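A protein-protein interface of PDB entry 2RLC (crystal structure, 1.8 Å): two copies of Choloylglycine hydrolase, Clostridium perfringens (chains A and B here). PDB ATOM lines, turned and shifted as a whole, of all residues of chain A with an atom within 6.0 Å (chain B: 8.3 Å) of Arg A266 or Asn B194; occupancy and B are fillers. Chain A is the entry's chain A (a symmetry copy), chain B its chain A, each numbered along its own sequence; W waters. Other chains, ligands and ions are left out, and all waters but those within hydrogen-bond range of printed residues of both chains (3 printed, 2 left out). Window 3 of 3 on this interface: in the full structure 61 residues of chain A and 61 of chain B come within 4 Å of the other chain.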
ATOM      1  N   GLY A 263       0.795 -21.182  -3.895  1.00  0.00           N
ATOM      2  CA  GLY A 263       2.224 -21.102  -3.601  1.00  0.00           C
ATOM      3  C   GLY A 263       3.164 -20.895  -4.776  1.00  0.00           C
ATOM      4  O   GLY A 263       4.222 -20.277  -4.616  1.00  0.00           O
ATOM      5  N   SER A 264       2.786 -21.406  -5.950  1.00  0.00           N
ATOM      6  CA  SER A 264       3.687 -21.445  -7.112  1.00  0.00           C
ATOM      7  C   SER A 264       3.494 -20.339  -8.155  1.00  0.00           C
ATOM      8  O   SER A 264       4.351 -20.147  -9.022  1.00  0.00           O
ATOM      9  CB  SER A 264       3.647 -22.823  -7.787  1.00  0.00           C
ATOM     10  OG  SER A 264       2.318 -23.275  -7.966  1.00  0.00           O
ATOM     11  N   THR A 265       2.368 -19.633  -8.083  1.00  0.00           N
ATOM     12  CA  THR A 265       2.117 -18.498  -8.969  1.00  0.00           C
ATOM     13  C   THR A 265       1.929 -17.261  -8.097  1.00  0.00           C
ATOM     14  O   THR A 265       0.804 -16.876  -7.763  1.00  0.00           O
ATOM     15  CB  THR A 265       0.900 -18.740  -9.899  1.00  0.00           C
ATOM     16  OG1 THR A 265       1.092 -19.954 -10.635  1.00  0.00           O
ATOM     17  CG2 THR A 265       0.726 -17.588 -10.889  1.00  0.00           C
ATOM     18  N   ARG A 266       3.052 -16.657  -7.720  1.00  0.00           N
ATOM     19  CA  ARG A 266       3.057 -15.558  -6.759  1.00  0.00           C
ATOM     20  C   ARG A 266       3.085 -14.205  -7.456  1.00  0.00           C
ATOM     21  O   ARG A 266       3.887 -13.982  -8.368  1.00  0.00           O
ATOM     22  CB  ARG A 266       4.249 -15.683  -5.803  1.00  0.00           C
ATOM     23  CG  ARG A 266       4.298 -16.985  -5.007  1.00  0.00           C
ATOM     24  CD  ARG A 266       3.356 -16.966  -3.814  1.00  0.00           C
ATOM     25  NE  ARG A 266       3.886 -16.159  -2.715  1.00  0.00           N
ATOM     26  CZ  ARG A 266       3.300 -16.016  -1.530  1.00  0.00           C
ATOM     27  NH1 ARG A 266       2.151 -16.625  -1.270  1.00  0.00           N
ATOM     28  NH2 ARG A 266       3.869 -15.259  -0.601  1.00  0.00           N
ATOM     29  N   THR A 267       2.205 -13.309  -7.013  1.00  0.00           N
ATOM     30  CA  THR A 267       2.123 -11.950  -7.552  1.00  0.00           C
ATOM     31  C   THR A 267       3.246 -11.079  -6.985  1.00  0.00           C
ATOM     32  O   THR A 267       3.960 -11.492  -6.066  1.00  0.00           O
ATOM     33  CB  THR A 267       0.759 -11.287  -7.234  1.00  0.00           C
ATOM     34  OG1 THR A 267       0.626 -11.110  -5.817  1.00  0.00           O
ATOM     35  CG2 THR A 267      -0.403 -12.134  -7.753  1.00  0.00           C
ATOM     36  N   VAL A 268       3.389  -9.876  -7.539  1.00  0.00           N
ATOM     37  CA  VAL A 268       4.367  -8.891  -7.069  1.00  0.00           C
ATOM     38  C   VAL A 268       4.058  -8.462  -5.627  1.00  0.00           C
ATOM     39  O   VAL A 268       4.965  -8.097  -4.869  1.00  0.00           O
ATOM     40  CB  VAL A 268       4.445  -7.672  -8.043  1.00  0.00           C
ATOM     41  CG1 VAL A 268       5.203  -6.504  -7.435  1.00  0.00           C
ATOM     42  CG2 VAL A 268       5.092  -8.087  -9.363  1.00  0.00           C
ATOM     43  N   GLU A 270       3.181 -10.463  -3.365  1.00  0.00           N
ATOM     44  CA  GLU A 270       3.428 -11.684  -2.581  1.00  0.00           C
ATOM     45  C   GLU A 270       2.148 -12.422  -2.164  1.00  0.00           C
ATOM     46  O   GLU A 270       2.030 -12.905  -1.032  1.00  0.00           O
ATOM     47  CB  GLU A 270       4.324 -11.392  -1.369  1.00  0.00           C
ATOM     48  CG  GLU A 270       5.786 -11.142  -1.719  1.00  0.00           C
ATOM     49  CD  GLU A 270       6.617 -10.750  -0.511  1.00  0.00           C
ATOM     50  OE1 GLU A 270       6.269  -9.752   0.157  1.00  0.00           O
ATOM     51  OE2 GLU A 270       7.621 -11.440  -0.234  1.00  0.00           O
ATOM     52  N   LYS A 271       1.198 -12.497  -3.091  1.00  0.00           N
ATOM     53  CA  LYS A 271      -0.024 -13.275  -2.906  1.00  0.00           C
ATOM     54  C   LYS A 271      -0.072 -14.411  -3.920  1.00  0.00           C
ATOM     55  O   LYS A 271       0.431 -14.275  -5.037  1.00  0.00           O
ATOM     56  CB  LYS A 271      -1.263 -12.389  -3.064  1.00  0.00           C
ATOM     57  CG  LYS A 271      -1.529 -11.455  -1.892  1.00  0.00           C
ATOM     58  CD  LYS A 271      -2.758 -10.594  -2.160  1.00  0.00           C
ATOM     59  CE  LYS A 271      -3.181  -9.805  -0.929  1.00  0.00           C
ATOM     60  NZ  LYS A 271      -3.767 -10.676   0.133  1.00  0.00           N
ATOM     61  N   SER A 272      -0.675 -15.528  -3.525  1.00  0.00           N
ATOM     62  CA  SER A 272      -0.831 -16.663  -4.427  1.00  0.00           C
ATOM     63  C   SER A 272      -2.007 -16.468  -5.370  1.00  0.00           C
ATOM     64  O   SER A 272      -3.148 -16.276  -4.942  1.00  0.00           O
ATOM     65  CB  SER A 272      -0.974 -17.975  -3.655  1.00  0.00           C
ATOM     66  OG  SER A 272       0.252 -18.333  -3.043  1.00  0.00           O
ATOM     67  N   ASP A 273      -1.706 -16.501  -6.662  1.00  0.00           N
ATOM     68  CA  ASP A 273      -2.723 -16.514  -7.693  1.00  0.00           C
ATOM     69  C   ASP A 273      -3.172 -17.961  -7.837  1.00  0.00           C
ATOM     70  O   ASP A 273      -2.361 -18.849  -8.096  1.00  0.00           O
ATOM     71  CB  ASP A 273      -2.135 -15.996  -9.007  1.00  0.00           C
ATOM     72  CG  ASP A 273      -3.196 -15.606 -10.018  1.00  0.00           C
ATOM     73  OD1 ASP A 273      -4.395 -15.580  -9.674  1.00  0.00           O
ATOM     74  OD2 ASP A 273      -2.817 -15.319 -11.173  1.00  0.00           O
ATOM     75  N   LEU B 191      14.178 -21.807 -11.963  1.00  0.00           N
ATOM     76  CA  LEU B 191      12.738 -21.577 -11.825  1.00  0.00           C
ATOM     77  C   LEU B 191      12.440 -20.610 -10.686  1.00  0.00           C
ATOM     78  O   LEU B 191      13.125 -20.617  -9.661  1.00  0.00           O
ATOM     79  CB  LEU B 191      11.989 -22.895 -11.593  1.00  0.00           C
ATOM     80  CG  LEU B 191      11.888 -23.938 -12.712  1.00  0.00           C
ATOM     81  CD1 LEU B 191      11.141 -25.158 -12.195  1.00  0.00           C
ATOM     82  CD2 LEU B 191      11.210 -23.386 -13.961  1.00  0.00           C
ATOM     83  N   ARG B 192      11.417 -19.781 -10.880  1.00  0.00           N
ATOM     84  CA  ARG B 192      10.990 -18.802  -9.880  1.00  0.00           C
ATOM     85  C   ARG B 192       9.472 -18.813  -9.723  1.00  0.00           C
ATOM     86  O   ARG B 192       8.739 -18.810 -10.714  1.00  0.00           O
ATOM     87  CB  ARG B 192      11.468 -17.399 -10.268  1.00  0.00           C
ATOM     88  CG  ARG B 192      12.963 -17.173 -10.088  1.00  0.00           C
ATOM     89  CD  ARG B 192      13.371 -15.771 -10.501  1.00  0.00           C
ATOM     90  NE  ARG B 192      13.443 -15.617 -11.954  1.00  0.00           N
ATOM     91  CZ  ARG B 192      13.849 -14.513 -12.576  1.00  0.00           C
ATOM     92  NH1 ARG B 192      14.225 -13.444 -11.879  1.00  0.00           N
ATOM     93  NH2 ARG B 192      13.880 -14.476 -13.901  1.00  0.00           N
ATOM     94  N   TYR B 193       9.002 -18.828  -8.477  1.00  0.00           N
ATOM     95  CA  TYR B 193       7.563 -18.790  -8.202  1.00  0.00           C
ATOM     96  C   TYR B 193       7.033 -17.362  -8.268  1.00  0.00           C
ATOM     97  O   TYR B 193       5.866 -17.137  -8.607  1.00  0.00           O
ATOM     98  CB  TYR B 193       7.236 -19.422  -6.843  1.00  0.00           C
ATOM     99  CG  TYR B 193       7.917 -20.751  -6.603  1.00  0.00           C
ATOM    100  CD1 TYR B 193       7.793 -21.798  -7.520  1.00  0.00           C
ATOM    101  CD2 TYR B 193       8.682 -20.963  -5.460  1.00  0.00           C
ATOM    102  CE1 TYR B 193       8.422 -23.015  -7.309  1.00  0.00           C
ATOM    103  CE2 TYR B 193       9.313 -22.182  -5.234  1.00  0.00           C
ATOM    104  CZ  TYR B 193       9.177 -23.201  -6.163  1.00  0.00           C
ATOM    105  OH  TYR B 193       9.798 -24.407  -5.946  1.00  0.00           O
ATOM    106  N   ASN B 194       7.900 -16.407  -7.942  1.00  0.00           N
ATOM    107  CA  ASN B 194       7.551 -14.992  -7.970  1.00  0.00           C
ATOM    108  C   ASN B 194       7.513 -14.442  -9.388  1.00  0.00           C
ATOM    109  O   ASN B 194       8.387 -14.738 -10.206  1.00  0.00           O
ATOM    110  CB  ASN B 194       8.529 -14.177  -7.120  1.00  0.00           C
ATOM    111  CG  ASN B 194       8.351 -14.415  -5.634  1.00  0.00           C
ATOM    112  OD1 ASN B 194       9.237 -14.953  -4.972  1.00  0.00           O
ATOM    113  ND2 ASN B 194       7.203 -14.011  -5.102  1.00  0.00           N
ATOM    114  N   GLN B 195       6.496 -13.629  -9.661  1.00  0.00           N
ATOM    115  CA  GLN B 195       6.300 -13.024 -10.974  1.00  0.00           C
ATOM    116  C   GLN B 195       7.518 -12.225 -11.439  1.00  0.00           C
ATOM    117  O   GLN B 195       8.164 -11.536 -10.643  1.00  0.00           O
ATOM    118  CB  GLN B 195       5.044 -12.137 -10.957  1.00  0.00           C
ATOM    119  CG  GLN B 195       4.723 -11.404 -12.266  1.00  0.00           C
ATOM    120  CD  GLN B 195       4.162 -12.305 -13.361  1.00  0.00           C
ATOM    121  OE1 GLN B 195       4.373 -13.521 -13.368  1.00  0.00           O
ATOM    122  NE2 GLN B 195       3.451 -11.700 -14.305  1.00  0.00           N
ATOM    123  N   VAL B 196       7.836 -12.356 -12.725  1.00  0.00           N
ATOM    124  CA  VAL B 196       8.795 -11.480 -13.392  1.00  0.00           C
ATOM    125  C   VAL B 196       7.983 -10.537 -14.289  1.00  0.00           C
ATOM    126  O   VAL B 196       7.596 -10.914 -15.397  1.00  0.00           O
ATOM    127  CB  VAL B 196       9.837 -12.271 -14.226  1.00  0.00           C
ATOM    128  CG1 VAL B 196      10.899 -11.329 -14.795  1.00  0.00           C
ATOM    129  CG2 VAL B 196      10.497 -13.357 -13.384  1.00  0.00           C
ATOM    130  N   PRO B 197       7.700  -9.313 -13.800  1.00  0.00           N
ATOM    131  CA  PRO B 197       6.789  -8.409 -14.504  1.00  0.00           C
ATOM    132  C   PRO B 197       7.361  -7.755 -15.765  1.00  0.00           C
ATOM    133  O   PRO B 197       6.595  -7.426 -16.674  1.00  0.00           O
ATOM    134  CB  PRO B 197       6.458  -7.348 -13.449  1.00  0.00           C
ATOM    135  CG  PRO B 197       7.622  -7.341 -12.535  1.00  0.00           C
ATOM    136  CD  PRO B 197       8.210  -8.723 -12.548  1.00  0.00           C
ATOM    137  N   GLY B 210       0.932 -12.288 -18.598  1.00  0.00           N
ATOM    138  CA  GLY B 210       0.122 -12.683 -17.452  1.00  0.00           C
ATOM    139  C   GLY B 210       1.010 -13.184 -16.330  1.00  0.00           C
ATOM    140  O   GLY B 210       2.238 -13.089 -16.410  1.00  0.00           O
ATOM    141  N   GLN B 211       0.387 -13.715 -15.282  1.00  0.00           N
ATOM    142  CA  GLN B 211       1.113 -14.274 -14.144  1.00  0.00           C
ATOM    143  C   GLN B 211       1.780 -15.598 -14.512  1.00  0.00           C
ATOM    144  O   GLN B 211       1.283 -16.331 -15.369  1.00  0.00           O
ATOM    145  CB  GLN B 211       0.166 -14.480 -12.956  1.00  0.00           C
ATOM    146  CG  GLN B 211      -0.344 -13.192 -12.310  1.00  0.00           C
ATOM    147  CD  GLN B 211       0.728 -12.443 -11.531  1.00  0.00           C
ATOM    148  OE1 GLN B 211       1.691 -13.034 -11.038  1.00  0.00           O
ATOM    149  NE2 GLN B 211       0.557 -11.133 -11.408  1.00  0.00           N
ATOM    150  N   GLY B 212       2.910 -15.889 -13.868  1.00  0.00           N
ATOM    151  CA  GLY B 212       3.583 -17.179 -14.026  1.00  0.00           C
ATOM    152  C   GLY B 212       4.833 -17.186 -14.890  1.00  0.00           C
ATOM    153  O   GLY B 212       5.343 -18.250 -15.243  1.00  0.00           O
ATOM    154  N   THR B 213       5.342 -16.003 -15.218  1.00  0.00           N
ATOM    155  CA  THR B 213       6.506 -15.884 -16.106  1.00  0.00           C
ATOM    156  C   THR B 213       7.794 -16.482 -15.530  1.00  0.00           C
ATOM    157  O   THR B 213       8.709 -16.834 -16.276  1.00  0.00           O
ATOM    158  CB  THR B 213       6.755 -14.419 -16.513  1.00  0.00           C
ATOM    159  OG1 THR B 213       6.887 -13.608 -15.339  1.00  0.00           O
ATOM    160  CG2 THR B 213       5.598 -13.901 -17.364  1.00  0.00           C
ATOM    161  N   GLY B 214       7.855 -16.598 -14.206  1.00  0.00           N
ATOM    162  CA  GLY B 214       9.028 -17.147 -13.525  1.00  0.00           C
ATOM    163  C   GLY B 214       9.234 -18.637 -13.738  1.00  0.00           C
ATOM    164  O   GLY B 214      10.359 -19.129 -13.646  1.00  0.00           O
ATOM    165  N   LEU B 215       8.145 -19.352 -14.020  1.00  0.00           N
ATOM    166  CA  LEU B 215       8.187 -20.804 -14.194  1.00  0.00           C
ATOM    167  C   LEU B 215       8.294 -21.263 -15.647  1.00  0.00           C
ATOM    168  O   LEU B 215       8.227 -22.463 -15.927  1.00  0.00           O
ATOM    169  CB  LEU B 215       6.972 -21.468 -13.531  1.00  0.00           C
ATOM    170  CG  LEU B 215       6.932 -21.656 -12.012  1.00  0.00           C
ATOM    171  CD1 LEU B 215       5.712 -22.490 -11.630  1.00  0.00           C
ATOM    172  CD2 LEU B 215       8.203 -22.302 -11.471  1.00  0.00           C
ATOM    173  N   ALA B 237       7.024 -25.040  -3.507  1.00  0.00           N
ATOM    174  CA  ALA B 237       6.457 -23.693  -3.505  1.00  0.00           C
ATOM    175  C   ALA B 237       5.409 -23.519  -2.419  1.00  0.00           C
ATOM    176  O   ALA B 237       5.347 -22.479  -1.765  1.00  0.00           O
ATOM    177  CB  ALA B 237       5.852 -23.374  -4.858  1.00  0.00           C
ATOM    178  N   MET B 238       4.578 -24.536  -2.235  1.00  0.00           N
ATOM    179  CA  MET B 238       3.521 -24.436  -1.247  1.00  0.00           C
ATOM    180  C   MET B 238       4.060 -24.540   0.177  1.00  0.00           C
ATOM    181  O   MET B 238       3.559 -23.869   1.071  1.00  0.00           O
ATOM    182  CB  MET B 238       2.439 -25.469  -1.495  1.00  0.00           C
ATOM    183  CG  MET B 238       1.120 -25.084  -0.868  1.00  0.00           C
ATOM    184  SD  MET B 238       0.012 -26.627  -0.860  1.00  0.00           S
ATOM    185  CE  MET B 238      -0.450 -26.674  -2.746  1.00  0.00           C
ATOM    186  N   LYS B 240       7.125 -23.582   1.037  1.00  0.00           N
ATOM    187  CA  LYS B 240       7.830 -22.307   1.196  1.00  0.00           C
ATOM    188  C   LYS B 240       6.906 -21.138   1.506  1.00  0.00           C
ATOM    189  O   LYS B 240       7.186 -20.334   2.399  1.00  0.00           O
ATOM    190  CB  LYS B 240       8.633 -21.979  -0.063  1.00  0.00           C
ATOM    191  CG  LYS B 240       9.974 -22.657  -0.128  1.00  0.00           C
ATOM    192  CD  LYS B 240      10.703 -22.299  -1.402  1.00  0.00           C
ATOM    193  CE  LYS B 240      12.115 -22.843  -1.373  1.00  0.00           C
ATOM    194  NZ  LYS B 240      12.720 -22.853  -2.728  1.00  0.00           N
ATOM    195  N   ASN B 241       5.805 -21.051   0.764  1.00  0.00           N
ATOM    196  CA  ASN B 241       4.939 -19.879   0.809  1.00  0.00           C
ATOM    197  C   ASN B 241       3.647 -20.047   1.612  1.00  0.00           C
ATOM    198  O   ASN B 241       3.039 -19.054   2.014  1.00  0.00           O
ATOM    199  CB  ASN B 241       4.627 -19.401  -0.617  1.00  0.00           C
ATOM    200  CG  ASN B 241       5.867 -18.906  -1.357  1.00  0.00           C
ATOM    201  OD1 ASN B 241       6.027 -19.144  -2.555  1.00  0.00           O
ATOM    202  ND2 ASN B 241       6.747 -18.212  -0.644  1.00  0.00           N
ATOM    203  N   ASP B 242       3.241 -21.293   1.853  1.00  0.00           N
ATOM    204  CA  ASP B 242       1.931 -21.575   2.449  1.00  0.00           C
ATOM    205  C   ASP B 242       1.924 -22.743   3.439  1.00  0.00           C
ATOM    206  O   ASP B 242       0.924 -23.459   3.554  1.00  0.00           O
ATOM    207  CB  ASP B 242       0.904 -21.822   1.341  1.00  0.00           C
ATOM    208  CG  ASP B 242       0.663 -20.596   0.493  1.00  0.00           C
ATOM    209  OD1 ASP B 242      -0.091 -19.708   0.935  1.00  0.00           O
ATOM    210  OD2 ASP B 242       1.232 -20.519  -0.616  1.00  0.00           O
ATOM    211  N   SER B 245      -1.057 -23.144   5.883  1.00  0.00           N
ATOM    212  CA  SER B 245      -2.394 -23.297   5.305  1.00  0.00           C
ATOM    213  C   SER B 245      -2.581 -24.609   4.536  1.00  0.00           C
ATOM    214  O   SER B 245      -3.625 -24.823   3.912  1.00  0.00           O
ATOM    215  CB  SER B 245      -2.752 -22.092   4.424  1.00  0.00           C
ATOM    216  OG  SER B 245      -1.837 -21.935   3.357  1.00  0.00           O
HETATM  217  O   HOH W   1       1.458 -16.772   1.409  1.00  0.00           O
HETATM  218  O   HOH W   2       2.061  -9.381  -9.881  1.00  0.00           O
HETATM  219  O   HOH W   3       6.170 -14.582  -2.703  1.00  0.00           O
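The side-chain amide oxygen of Asn B241 lies close to the backbone carbonyl oxygen of Gly A263 (3.0 Å). OD2 of Asp B242 lies within hydrogen-bond range of OG of Ser A272 (3.4 Å). N of Gln B195 sits at hydrogen-bond distance from O of Arg A266. The backbone carbonyl oxygen (O) of Tyr B193 sits close to the backbone carbonyl oxygen (O) of Ser A264, at 3.4 Å. The backbone carbonyl oxygen (O) of Tyr B193 sits at hydrogen-bond distance from the backbone NH (N) of Arg A266. The backbone NH (N) of Gly A263 sits close to the side-chain carboxylate (OD2) of Asp B242 (3.4 Å).
Of chain B, only Tyr B193 (3.0 Å), Asn B194 (3.5 Å), Gln B195 (2.9 Å), Gln B211 (3.6 Å) and Asn B241 (3.6 Å) come within 4 Å of Arg A266. Printed residues of chain B within 4 Å of Thr A267: Gln B211. Printed residues of chain B within 4 Å of Asp A273: Gln B211 (3.5 Å). Asn B194 touches just one residue of chain A: Arg A266. Printed residues of chain A within 4 Å of Gln B195: Arg A266 (2.9 Å). Pro B197 touches none of the printed residues of chain A. Printed residues of chain A within 4 Å of Ala B237: Gly A263 (3.5 Å) and Ser A264 (3.7 Å). The nearest residue of chain A that does not touch Asn B194 is Thr A267 (4.2 Å).
Water W3 bridges ND2 of Asn B194 and NE of Arg A266. Water W2 bridges N of Val A268 (2.7 Å) and NE2 of Gln B211 (2.8 Å). Water W1 lies within hydrogen-bond range of NH1 of Arg A266 (2.8 Å), O of Asn B241 (2.8 Å) and OD1 of Asp B242 (3.4 Å).
Among the printed residues, pairs that only touch across the chains: Gly A263 with Tyr B193 (3.8 Å), Gly A263 with Ala B237 (3.5 Å), Ser A264 with Leu B215 (3.8 Å), Ser A264 with Ala B237 (3.7 Å), Thr A265 with Tyr B193 (3.97 Å), Thr A265 with Gln B211 (3.8 Å), Arg A266 with Asn B194 (3.5 Å), Arg A266 with Gln B211 (3.6 Å), Arg A266 with Asn B241 (3.6 Å), Thr A267 with Gln B211 (3.7 Å) and Asp A273 with Gln B211 (3.5 Å).
The side-chain hydroxyl of Thr A267 lies within hydrogen-bond range of the backbone NH of Lys A271, at 3.1 Å. O of Thr A265 is in hydrogen-bond range of N of Asp A273, 2.8 Å away. The side-chain amide nitrogen (NE2) of Gln B195 is in hydrogen-bond range of the backbone carbonyl oxygen (O) of Gly B210 (2.8 Å). The guanidinium group (NH1) of Arg A266 lies within hydrogen-bond range of the side-chain hydroxyl (OG) of Ser A272. The guanidinium group (NH2) of Arg A266 lies within hydrogen-bond range of the backbone carbonyl oxygen (O) of Glu A270, 3.0 Å away. N of Gly B212 lies within hydrogen-bond range of OE1 of Gln B195, 2.8 Å away.
Of the 19 printed residues of chain B, 8 touch a printed residue of chain A. Printed residues of chain B that touch a printed residue of chain A: Tyr B193, Asn B194, Gln B195, Gln B211, Leu B215, Ala B237, Asn B241 and Asp B242. Hydrophobic or aromatic side chains of chain B that line the printed part of chain A: Tyr B193, Leu B215 and Ala B237. Among the printed residues, 17 pairs touch across the chains.
No position is printed for both chains.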
